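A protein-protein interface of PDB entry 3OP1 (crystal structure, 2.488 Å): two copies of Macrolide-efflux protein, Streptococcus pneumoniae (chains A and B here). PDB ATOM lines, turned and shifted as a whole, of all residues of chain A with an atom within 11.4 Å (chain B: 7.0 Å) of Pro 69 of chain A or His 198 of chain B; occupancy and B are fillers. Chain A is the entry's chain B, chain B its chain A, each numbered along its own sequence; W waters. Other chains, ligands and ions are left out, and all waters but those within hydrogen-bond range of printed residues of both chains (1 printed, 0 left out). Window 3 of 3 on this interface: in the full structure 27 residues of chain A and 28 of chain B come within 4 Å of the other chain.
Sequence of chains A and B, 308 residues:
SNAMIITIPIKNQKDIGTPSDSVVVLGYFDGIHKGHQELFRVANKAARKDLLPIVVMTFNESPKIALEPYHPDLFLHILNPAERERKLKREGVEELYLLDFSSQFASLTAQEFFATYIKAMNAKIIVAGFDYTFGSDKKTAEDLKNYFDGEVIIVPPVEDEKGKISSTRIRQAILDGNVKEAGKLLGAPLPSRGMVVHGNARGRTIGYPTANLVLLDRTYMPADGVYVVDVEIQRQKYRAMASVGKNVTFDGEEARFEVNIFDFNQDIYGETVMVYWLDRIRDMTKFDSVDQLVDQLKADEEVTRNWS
The backbone NH (N) of Val 197 of chain B lies within hydrogen-bond range of the backbone carbonyl oxygen (O) of Asn 212 of chain B, at 3.0 Å.
Water W1 lies within hydrogen-bond range of the backbone carbonyl oxygen (O) of Glu 68 of chain A (2.8 Å), the backbone carbonyl oxygen (O) of Ile 65 of chain A (2.8 Å), the backbone NH (N) of His 198 of chain B (2.9 Å) and the backbone NH (N) of Tyr 70 of chain A (3.3 Å).
Hydrophobic or aromatic side chains of chain A that line the printed part of chain B: Ile 65, Ala 66, Tyr 70 and Phe 75.
Among the printed residues, no Asp or Glu carboxylate lies within 4 Å of a Lys or Arg side-chain nitrogen of the other chain.
Among the printed residues, pairs that only touch across the chains: Ile 65 of chain A with Met 195 of chain B (2.9 Å), Ile 65 of chain A with His 198 of chain B (3.6 Å), Ala 66 of chain A with Tyr 269 of chain B (3.4 Å), Glu 68 of chain A with His 198 of chain B (3.4 Å), Pro 69 of chain A with His 198 of chain B (3.8 Å), Tyr 70 of chain A with Val 197 of chain B (2.9 Å), Tyr 70 of chain A with Arg 256 of chain B (3.6 Å), Phe 75 of chain A with Met 195 of chain B (3.4 Å) and Ser 102 of chain A with Tyr 269 of chain B (3.3 Å).
The backbone NH (N) of Ser 103 of chain A lies within hydrogen-bond range of the backbone carbonyl oxygen (O) of Tyr 269 of chain B.
O of Ala 66 of chain A is in hydrogen-bond range of NE2 of His 198 of chain B.
The backbone carbonyl oxygen (O) of His 198 of chain B is in hydrogen-bond range of the backbone NH (N) of Tyr 70 of chain A, at 2.8 Å.
Val 197 of chain B touches just one residue of chain A: Tyr 70 (2.9 Å).
No residue of chain A comes within 4 Å of Asn 212 of chain B.
Of the printed residues of chain B, Glu 68 of chain A touches His 198.
Printed residues of chain A within 4 Å of Tyr 269 of chain B: Ala 66, Ser 102 and Ser 103.
Of the printed residues of chain A, Met 195 of chain B touches Ile 65 (2.9 Å) and Phe 75 (3.4 Å).
Of the printed residues of chain B, Ala 66 of chain A touches His 198 and Tyr 269.
Of the printed residues of chain A, Arg 256 of chain B touches Tyr 70 (3.6 Å).
The nearest residue of chain A that does not touch His 198 of chain B is Leu 67 of chain A (4.2 Å).
No position is printed for both chains.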
ATOM      1  N   SER A  62     -28.762 -32.177  22.557  1.00  0.00           N
ATOM      2  CA  SER A  62     -28.053 -32.711  21.424  1.00  0.00           C
ATOM      3  C   SER A  62     -26.780 -31.911  21.143  1.00  0.00           C
ATOM      4  O   SER A  62     -26.788 -30.689  21.162  1.00  0.00           O
ATOM      5  CB  SER A  62     -28.959 -32.741  20.205  1.00  0.00           C
ATOM      6  OG  SER A  62     -28.254 -33.211  19.067  1.00  0.00           O
ATOM      7  N   PRO A  63     -25.657 -32.607  20.935  1.00  0.00           N
ATOM      8  CA  PRO A  63     -24.446 -31.921  20.468  1.00  0.00           C
ATOM      9  C   PRO A  63     -24.738 -31.265  19.125  1.00  0.00           C
ATOM     10  O   PRO A  63     -24.082 -30.277  18.729  1.00  0.00           O
ATOM     11  CB  PRO A  63     -23.415 -33.045  20.319  1.00  0.00           C
ATOM     12  CG  PRO A  63     -24.120 -34.317  20.759  1.00  0.00           C
ATOM     13  CD  PRO A  63     -25.368 -33.945  21.474  1.00  0.00           C
ATOM     14  N   LYS A  64     -25.738 -31.803  18.428  1.00  0.00           N
ATOM     15  CA  LYS A  64     -26.136 -31.240  17.139  1.00  0.00           C
ATOM     16  C   LYS A  64     -26.430 -29.720  17.203  1.00  0.00           C
ATOM     17  O   LYS A  64     -26.378 -29.032  16.189  1.00  0.00           O
ATOM     18  CB  LYS A  64     -27.314 -32.029  16.539  1.00  0.00           C
ATOM     19  CG  LYS A  64     -26.924 -33.270  15.731  1.00  0.00           C
ATOM     20  CD  LYS A  64     -28.173 -34.049  15.295  1.00  0.00           C
ATOM     21  CE  LYS A  64     -27.975 -34.779  13.950  1.00  0.00           C
ATOM     22  NZ  LYS A  64     -29.289 -35.088  13.276  1.00  0.00           N
ATOM     23  N   ILE A  65     -26.704 -29.196  18.397  1.00  0.00           N
ATOM     24  CA  ILE A  65     -27.103 -27.795  18.535  1.00  0.00           C
ATOM     25  C   ILE A  65     -25.950 -26.811  18.478  1.00  0.00           C
ATOM     26  O   ILE A  65     -26.123 -25.681  18.013  1.00  0.00           O
ATOM     27  CB  ILE A  65     -27.924 -27.557  19.811  1.00  0.00           C
ATOM     28  CG1 ILE A  65     -29.341 -28.098  19.611  1.00  0.00           C
ATOM     29  CG2 ILE A  65     -27.915 -26.045  20.198  1.00  0.00           C
ATOM     30  CD1 ILE A  65     -30.136 -28.224  20.868  1.00  0.00           C
ATOM     31  N   ALA A  66     -24.778 -27.235  18.943  1.00  0.00           N
ATOM     32  CA  ALA A  66     -23.589 -26.396  18.852  1.00  0.00           C
ATOM     33  C   ALA A  66     -23.025 -26.492  17.455  1.00  0.00           C
ATOM     34  O   ALA A  66     -22.289 -25.608  17.011  1.00  0.00           O
ATOM     35  CB  ALA A  66     -22.550 -26.816  19.869  1.00  0.00           C
ATOM     36  N   LEU A  67     -23.407 -27.547  16.748  1.00  0.00           N
ATOM     37  CA  LEU A  67     -22.818 -27.833  15.444  1.00  0.00           C
ATOM     38  C   LEU A  67     -23.655 -27.481  14.236  1.00  0.00           C
ATOM     39  O   LEU A  67     -23.099 -27.104  13.224  1.00  0.00           O
ATOM     40  CB  LEU A  67     -22.404 -29.293  15.344  1.00  0.00           C
ATOM     41  CG  LEU A  67     -21.390 -29.701  16.418  1.00  0.00           C
ATOM     42  CD1 LEU A  67     -21.117 -31.199  16.416  1.00  0.00           C
ATOM     43  CD2 LEU A  67     -20.114 -28.928  16.249  1.00  0.00           C
ATOM     44  N   GLU A  68     -24.972 -27.606  14.286  1.00  0.00           N
ATOM     45  CA  GLU A  68     -25.721 -27.331  13.057  1.00  0.00           C
ATOM     46  C   GLU A  68     -26.701 -26.150  13.110  1.00  0.00           C
ATOM     47  O   GLU A  68     -26.955 -25.584  14.163  1.00  0.00           O
ATOM     48  CB  GLU A  68     -26.453 -28.570  12.562  1.00  0.00           C
ATOM     49  CG  GLU A  68     -25.671 -29.826  12.651  1.00  0.00           C
ATOM     50  CD  GLU A  68     -26.596 -31.026  12.713  1.00  0.00           C
ATOM     51  OE1 GLU A  68     -27.816 -30.803  12.903  1.00  0.00           O
ATOM     52  OE2 GLU A  68     -26.117 -32.178  12.564  1.00  0.00           O
ATOM     53  N   PRO A  69     -27.255 -25.780  11.946  1.00  0.00           N
ATOM     54  CA  PRO A  69     -28.278 -24.742  11.910  1.00  0.00           C
ATOM     55  C   PRO A  69     -29.370 -25.119  12.864  1.00  0.00           C
ATOM     56  O   PRO A  69     -29.830 -26.266  12.890  1.00  0.00           O
ATOM     57  CB  PRO A  69     -28.808 -24.818  10.478  1.00  0.00           C
ATOM     58  CG  PRO A  69     -27.678 -25.401   9.684  1.00  0.00           C
ATOM     59  CD  PRO A  69     -27.015 -26.364  10.611  1.00  0.00           C
ATOM     60  N   TYR A  70     -29.774 -24.148  13.659  1.00  0.00           N
ATOM     61  CA  TYR A  70     -30.812 -24.370  14.628  1.00  0.00           C
ATOM     62  C   TYR A  70     -32.118 -24.899  14.036  1.00  0.00           C
ATOM     63  O   TYR A  70     -32.524 -24.502  12.958  1.00  0.00           O
ATOM     64  CB  TYR A  70     -31.114 -23.082  15.362  1.00  0.00           C
ATOM     65  CG  TYR A  70     -32.308 -23.311  16.202  1.00  0.00           C
ATOM     66  CD1 TYR A  70     -32.261 -24.261  17.226  1.00  0.00           C
ATOM     67  CD2 TYR A  70     -33.497 -22.685  15.934  1.00  0.00           C
ATOM     68  CE1 TYR A  70     -33.367 -24.541  17.995  1.00  0.00           C
ATOM     69  CE2 TYR A  70     -34.631 -22.964  16.708  1.00  0.00           C
ATOM     70  CZ  TYR A  70     -34.540 -23.890  17.749  1.00  0.00           C
ATOM     71  OH  TYR A  70     -35.619 -24.207  18.528  1.00  0.00           O
ATOM     72  N   HIS A  71     -32.770 -25.801  14.760  1.00  0.00           N
ATOM     73  CA  HIS A  71     -34.125 -26.230  14.436  1.00  0.00           C
ATOM     74  C   HIS A  71     -34.692 -26.822  15.707  1.00  0.00           C
ATOM     75  O   HIS A  71     -34.020 -27.565  16.367  1.00  0.00           O
ATOM     76  CB  HIS A  71     -34.148 -27.281  13.310  1.00  0.00           C
ATOM     77  CG  HIS A  71     -35.534 -27.741  12.944  1.00  0.00           C
ATOM     78  ND1 HIS A  71     -36.309 -28.523  13.778  1.00  0.00           N
ATOM     79  CD2 HIS A  71     -36.281 -27.530  11.835  1.00  0.00           C
ATOM     80  CE1 HIS A  71     -37.474 -28.762  13.206  1.00  0.00           C
ATOM     81  NE2 HIS A  71     -37.482 -28.173  12.022  1.00  0.00           N
ATOM     82  N   PRO A  72     -35.942 -26.513  16.042  1.00  0.00           N
ATOM     83  CA  PRO A  72     -36.554 -26.982  17.298  1.00  0.00           C
ATOM     84  C   PRO A  72     -36.503 -28.501  17.504  1.00  0.00           C
ATOM     85  O   PRO A  72     -36.417 -28.967  18.639  1.00  0.00           O
ATOM     86  CB  PRO A  72     -38.006 -26.477  17.191  1.00  0.00           C
ATOM     87  CG  PRO A  72     -38.247 -26.305  15.735  1.00  0.00           C
ATOM     88  CD  PRO A  72     -36.901 -25.775  15.211  1.00  0.00           C
ATOM     89  N   ASP A  73     -36.527 -29.261  16.422  1.00  0.00           N
ATOM     90  CA  ASP A  73     -36.432 -30.710  16.502  1.00  0.00           C
ATOM     91  C   ASP A  73     -35.155 -31.164  17.237  1.00  0.00           C
ATOM     92  O   ASP A  73     -35.135 -32.194  17.891  1.00  0.00           O
ATOM     93  CB  ASP A  73     -36.496 -31.314  15.115  1.00  0.00           C
ATOM     94  CG  ASP A  73     -37.927 -31.516  14.634  1.00  0.00           C
ATOM     95  OD1 ASP A  73     -38.845 -30.908  15.221  1.00  0.00           O
ATOM     96  OD2 ASP A  73     -38.135 -32.304  13.678  1.00  0.00           O
ATOM     97  N   LEU A  74     -34.106 -30.370  17.125  1.00  0.00           N
ATOM     98  CA  LEU A  74     -32.885 -30.616  17.850  1.00  0.00           C
ATOM     99  C   LEU A  74     -33.063 -30.696  19.351  1.00  0.00           C
ATOM    100  O   LEU A  74     -32.230 -31.293  20.013  1.00  0.00           O
ATOM    101  CB  LEU A  74     -31.891 -29.510  17.568  1.00  0.00           C
ATOM    102  CG  LEU A  74     -31.423 -29.383  16.134  1.00  0.00           C
ATOM    103  CD1 LEU A  74     -30.300 -28.383  16.156  1.00  0.00           C
ATOM    104  CD2 LEU A  74     -30.960 -30.731  15.587  1.00  0.00           C
ATOM    105  N   PHE A  75     -34.115 -30.101  19.906  1.00  0.00           N
ATOM    106  CA  PHE A  75     -34.285 -30.170  21.357  1.00  0.00           C
ATOM    107  C   PHE A  75     -35.063 -31.387  21.834  1.00  0.00           C
ATOM    108  O   PHE A  75     -35.366 -31.517  23.019  1.00  0.00           O
ATOM    109  CB  PHE A  75     -34.985 -28.950  21.869  1.00  0.00           C
ATOM    110  CG  PHE A  75     -34.100 -27.805  22.095  1.00  0.00           C
ATOM    111  CD1 PHE A  75     -33.687 -27.487  23.380  1.00  0.00           C
ATOM    112  CD2 PHE A  75     -33.723 -26.985  21.048  1.00  0.00           C
ATOM    113  CE1 PHE A  75     -32.873 -26.368  23.606  1.00  0.00           C
ATOM    114  CE2 PHE A  75     -32.918 -25.876  21.277  1.00  0.00           C
ATOM    115  CZ  PHE A  75     -32.493 -25.571  22.558  1.00  0.00           C
ATOM    116  N   PHE A 101     -22.985 -29.214  25.652  1.00  0.00           N
ATOM    117  CA  PHE A 101     -22.029 -29.485  24.612  1.00  0.00           C
ATOM    118  C   PHE A 101     -21.807 -28.185  23.866  1.00  0.00           C
ATOM    119  O   PHE A 101     -22.358 -27.948  22.802  1.00  0.00           O
ATOM    120  CB  PHE A 101     -22.558 -30.560  23.673  1.00  0.00           C
ATOM    121  CG  PHE A 101     -21.582 -30.977  22.628  1.00  0.00           C
ATOM    122  CD1 PHE A 101     -20.857 -32.134  22.768  1.00  0.00           C
ATOM    123  CD2 PHE A 101     -21.383 -30.209  21.512  1.00  0.00           C
ATOM    124  CE1 PHE A 101     -19.961 -32.516  21.812  1.00  0.00           C
ATOM    125  CE2 PHE A 101     -20.488 -30.591  20.554  1.00  0.00           C
ATOM    126  CZ  PHE A 101     -19.777 -31.745  20.704  1.00  0.00           C
ATOM    127  N   SER A 102     -20.987 -27.339  24.465  1.00  0.00           N
ATOM    128  CA  SER A 102     -20.659 -26.030  23.934  1.00  0.00           C
ATOM    129  C   SER A 102     -19.641 -26.101  22.818  1.00  0.00           C
ATOM    130  O   SER A 102     -19.055 -27.134  22.576  1.00  0.00           O
ATOM    131  CB  SER A 102     -20.162 -25.113  25.043  1.00  0.00           C
ATOM    132  OG  SER A 102     -18.986 -25.611  25.631  1.00  0.00           O
ATOM    133  N   SER A 103     -19.451 -24.982  22.138  1.00  0.00           N
ATOM    134  CA  SER A 103     -18.469 -24.881  21.082  1.00  0.00           C
ATOM    135  C   SER A 103     -17.108 -25.170  21.689  1.00  0.00           C
ATOM    136  O   SER A 103     -16.267 -25.810  21.081  1.00  0.00           O
ATOM    137  CB  SER A 103     -18.482 -23.473  20.503  1.00  0.00           C
ATOM    138  OG  SER A 103     -19.359 -23.371  19.405  1.00  0.00           O
ATOM    139  N   GLN A 104     -16.896 -24.678  22.899  1.00  0.00           N
ATOM    140  CA  GLN A 104     -15.659 -24.891  23.623  1.00  0.00           C
ATOM    141  C   GLN A 104     -15.402 -26.366  23.903  1.00  0.00           C
ATOM    142  O   GLN A 104     -14.301 -26.855  23.726  1.00  0.00           O
ATOM    143  CB  GLN A 104     -15.667 -24.121  24.932  1.00  0.00           C
ATOM    144  CG  GLN A 104     -14.624 -24.597  25.922  1.00  0.00           C
ATOM    145  CD  GLN A 104     -14.280 -23.508  26.917  1.00  0.00           C
ATOM    146  OE1 GLN A 104     -14.802 -22.393  26.819  1.00  0.00           O
ATOM    147  NE2 GLN A 104     -13.410 -23.813  27.875  1.00  0.00           N
ATOM    148  N   ALA A 106     -16.473 -28.715  22.173  1.00  0.00           N
ATOM    149  CA  ALA A 106     -16.266 -29.348  20.881  1.00  0.00           C
ATOM    150  C   ALA A 106     -14.785 -29.307  20.500  1.00  0.00           C
ATOM    151  O   ALA A 106     -14.252 -30.249  19.904  1.00  0.00           O
ATOM    152  CB  ALA A 106     -17.098 -28.659  19.824  1.00  0.00           C
ATOM    153  N   MET B 195     -30.298 -20.634  25.533  1.00  0.00           N
ATOM    154  CA  MET B 195     -29.208 -21.328  24.878  1.00  0.00           C
ATOM    155  C   MET B 195     -28.761 -20.727  23.549  1.00  0.00           C
ATOM    156  O   MET B 195     -29.595 -20.464  22.673  1.00  0.00           O
ATOM    157  CB  MET B 195     -29.574 -22.772  24.649  1.00  0.00           C
ATOM    158  CG  MET B 195     -28.383 -23.555  24.026  1.00  0.00           C
ATOM    159  SD  MET B 195     -28.501 -25.423  24.502  1.00  0.00           S
ATOM    160  CE  MET B 195     -29.139 -26.165  22.879  1.00  0.00           C
ATOM    161  N   VAL B 196     -27.455 -20.575  23.366  1.00  0.00           N
ATOM    162  CA  VAL B 196     -26.927 -20.064  22.112  1.00  0.00           C
ATOM    163  C   VAL B 196     -27.108 -21.089  21.010  1.00  0.00           C
ATOM    164  O   VAL B 196     -26.785 -22.247  21.166  1.00  0.00           O
ATOM    165  CB  VAL B 196     -25.455 -19.652  22.211  1.00  0.00           C
ATOM    166  CG1 VAL B 196     -24.992 -19.068  20.901  1.00  0.00           C
ATOM    167  CG2 VAL B 196     -25.265 -18.655  23.316  1.00  0.00           C
ATOM    168  N   VAL B 197     -27.627 -20.617  19.890  1.00  0.00           N
ATOM    169  CA  VAL B 197     -28.040 -21.435  18.775  1.00  0.00           C
ATOM    170  C   VAL B 197     -27.545 -20.841  17.463  1.00  0.00           C
ATOM    171  O   VAL B 197     -27.237 -19.661  17.389  1.00  0.00           O
ATOM    172  CB  VAL B 197     -29.573 -21.495  18.740  1.00  0.00           C
ATOM    173  CG1 VAL B 197     -30.094 -21.287  17.354  1.00  0.00           C
ATOM    174  CG2 VAL B 197     -30.081 -22.762  19.348  1.00  0.00           C
ATOM    175  N   HIS B 198     -27.473 -21.658  16.422  1.00  0.00           N
ATOM    176  CA  HIS B 198     -27.061 -21.156  15.126  1.00  0.00           C
ATOM    177  C   HIS B 198     -28.292 -20.659  14.391  1.00  0.00           C
ATOM    178  O   HIS B 198     -29.117 -21.436  13.939  1.00  0.00           O
ATOM    179  CB  HIS B 198     -26.414 -22.265  14.306  1.00  0.00           C
ATOM    180  CG  HIS B 198     -25.021 -22.612  14.727  1.00  0.00           C
ATOM    181  ND1 HIS B 198     -23.916 -21.930  14.278  1.00  0.00           N
ATOM    182  CD2 HIS B 198     -24.556 -23.592  15.532  1.00  0.00           C
ATOM    183  CE1 HIS B 198     -22.829 -22.467  14.799  1.00  0.00           C
ATOM    184  NE2 HIS B 198     -23.191 -23.476  15.565  1.00  0.00           N
ATOM    185  N   GLY B 199     -28.391 -19.348  14.265  1.00  0.00           N
ATOM    186  CA  GLY B 199     -29.501 -18.695  13.608  1.00  0.00           C
ATOM    187  C   GLY B 199     -28.923 -17.456  12.977  1.00  0.00           C
ATOM    188  O   GLY B 199     -27.817 -17.077  13.325  1.00  0.00           O
ATOM    189  N   ASN B 200     -29.629 -16.839  12.044  1.00  0.00           N
ATOM    190  CA  ASN B 200     -29.122 -15.628  11.415  1.00  0.00           C
ATOM    191  C   ASN B 200     -27.840 -15.142  12.086  1.00  0.00           C
ATOM    192  O   ASN B 200     -27.423 -14.001  11.921  1.00  0.00           O
ATOM    193  CB  ASN B 200     -30.181 -14.530  11.438  1.00  0.00           C
ATOM    194  CG  ASN B 200     -30.208 -13.775  12.746  1.00  0.00           C
ATOM    195  OD1 ASN B 200     -31.203 -13.154  13.091  1.00  0.00           O
ATOM    196  ND2 ASN B 200     -29.108 -13.820  13.475  1.00  0.00           N
ATOM    197  N   ASN B 212     -27.880 -15.419  18.899  1.00  0.00           N
ATOM    198  CA  ASN B 212     -29.254 -15.950  18.921  1.00  0.00           C
ATOM    199  C   ASN B 212     -29.542 -16.889  20.060  1.00  0.00           C
ATOM    200  O   ASN B 212     -28.993 -17.983  20.092  1.00  0.00           O
ATOM    201  CB  ASN B 212     -29.530 -16.727  17.635  1.00  0.00           C
ATOM    202  CG  ASN B 212     -29.026 -15.999  16.425  1.00  0.00           C
ATOM    203  OD1 ASN B 212     -28.068 -16.438  15.773  1.00  0.00           O
ATOM    204  ND2 ASN B 212     -29.624 -14.852  16.141  1.00  0.00           N
ATOM    205  N   ARG B 256     -37.488 -16.712  21.078  1.00  0.00           N
ATOM    206  CA  ARG B 256     -36.118 -16.508  20.704  1.00  0.00           C
ATOM    207  C   ARG B 256     -35.885 -15.017  20.710  1.00  0.00           C
ATOM    208  O   ARG B 256     -36.790 -14.196  20.471  1.00  0.00           O
ATOM    209  CB  ARG B 256     -35.846 -17.037  19.292  1.00  0.00           C
ATOM    210  CG  ARG B 256     -36.233 -18.469  19.086  1.00  0.00           C
ATOM    211  CD  ARG B 256     -35.988 -18.832  17.673  1.00  0.00           C
ATOM    212  NE  ARG B 256     -34.680 -18.341  17.250  1.00  0.00           N
ATOM    213  CZ  ARG B 256     -34.132 -18.607  16.065  1.00  0.00           C
ATOM    214  NH1 ARG B 256     -32.937 -18.117  15.782  1.00  0.00           N
ATOM    215  NH2 ARG B 256     -34.764 -19.375  15.169  1.00  0.00           N
ATOM    216  N   TYR B 269     -21.719 -21.427  21.009  1.00  0.00           N
ATOM    217  CA  TYR B 269     -22.908 -22.145  20.592  1.00  0.00           C
ATOM    218  C   TYR B 269     -23.148 -23.367  21.453  1.00  0.00           C
ATOM    219  O   TYR B 269     -22.222 -24.064  21.818  1.00  0.00           O
ATOM    220  CB  TYR B 269     -22.786 -22.569  19.140  1.00  0.00           C
ATOM    221  CG  TYR B 269     -22.542 -21.425  18.199  1.00  0.00           C
ATOM    222  CD1 TYR B 269     -23.595 -20.716  17.658  1.00  0.00           C
ATOM    223  CD2 TYR B 269     -21.258 -21.053  17.853  1.00  0.00           C
ATOM    224  CE1 TYR B 269     -23.376 -19.680  16.801  1.00  0.00           C
ATOM    225  CE2 TYR B 269     -21.034 -20.015  16.998  1.00  0.00           C
ATOM    226  CZ  TYR B 269     -22.096 -19.332  16.476  1.00  0.00           C
ATOM    227  OH  TYR B 269     -21.873 -18.294  15.617  1.00  0.00           O
ATOM    228  N   GLY B 270     -24.403 -23.609  21.791  1.00  0.00           N
ATOM    229  CA  GLY B 270     -24.768 -24.762  22.581  1.00  0.00           C
ATOM    230  C   GLY B 270     -24.536 -24.522  24.046  1.00  0.00           C
ATOM    231  O   GLY B 270     -24.751 -25.386  24.875  1.00  0.00           O
HETATM  232  O   HOH W   1     -28.041 -24.456  16.428  1.00  0.00           O
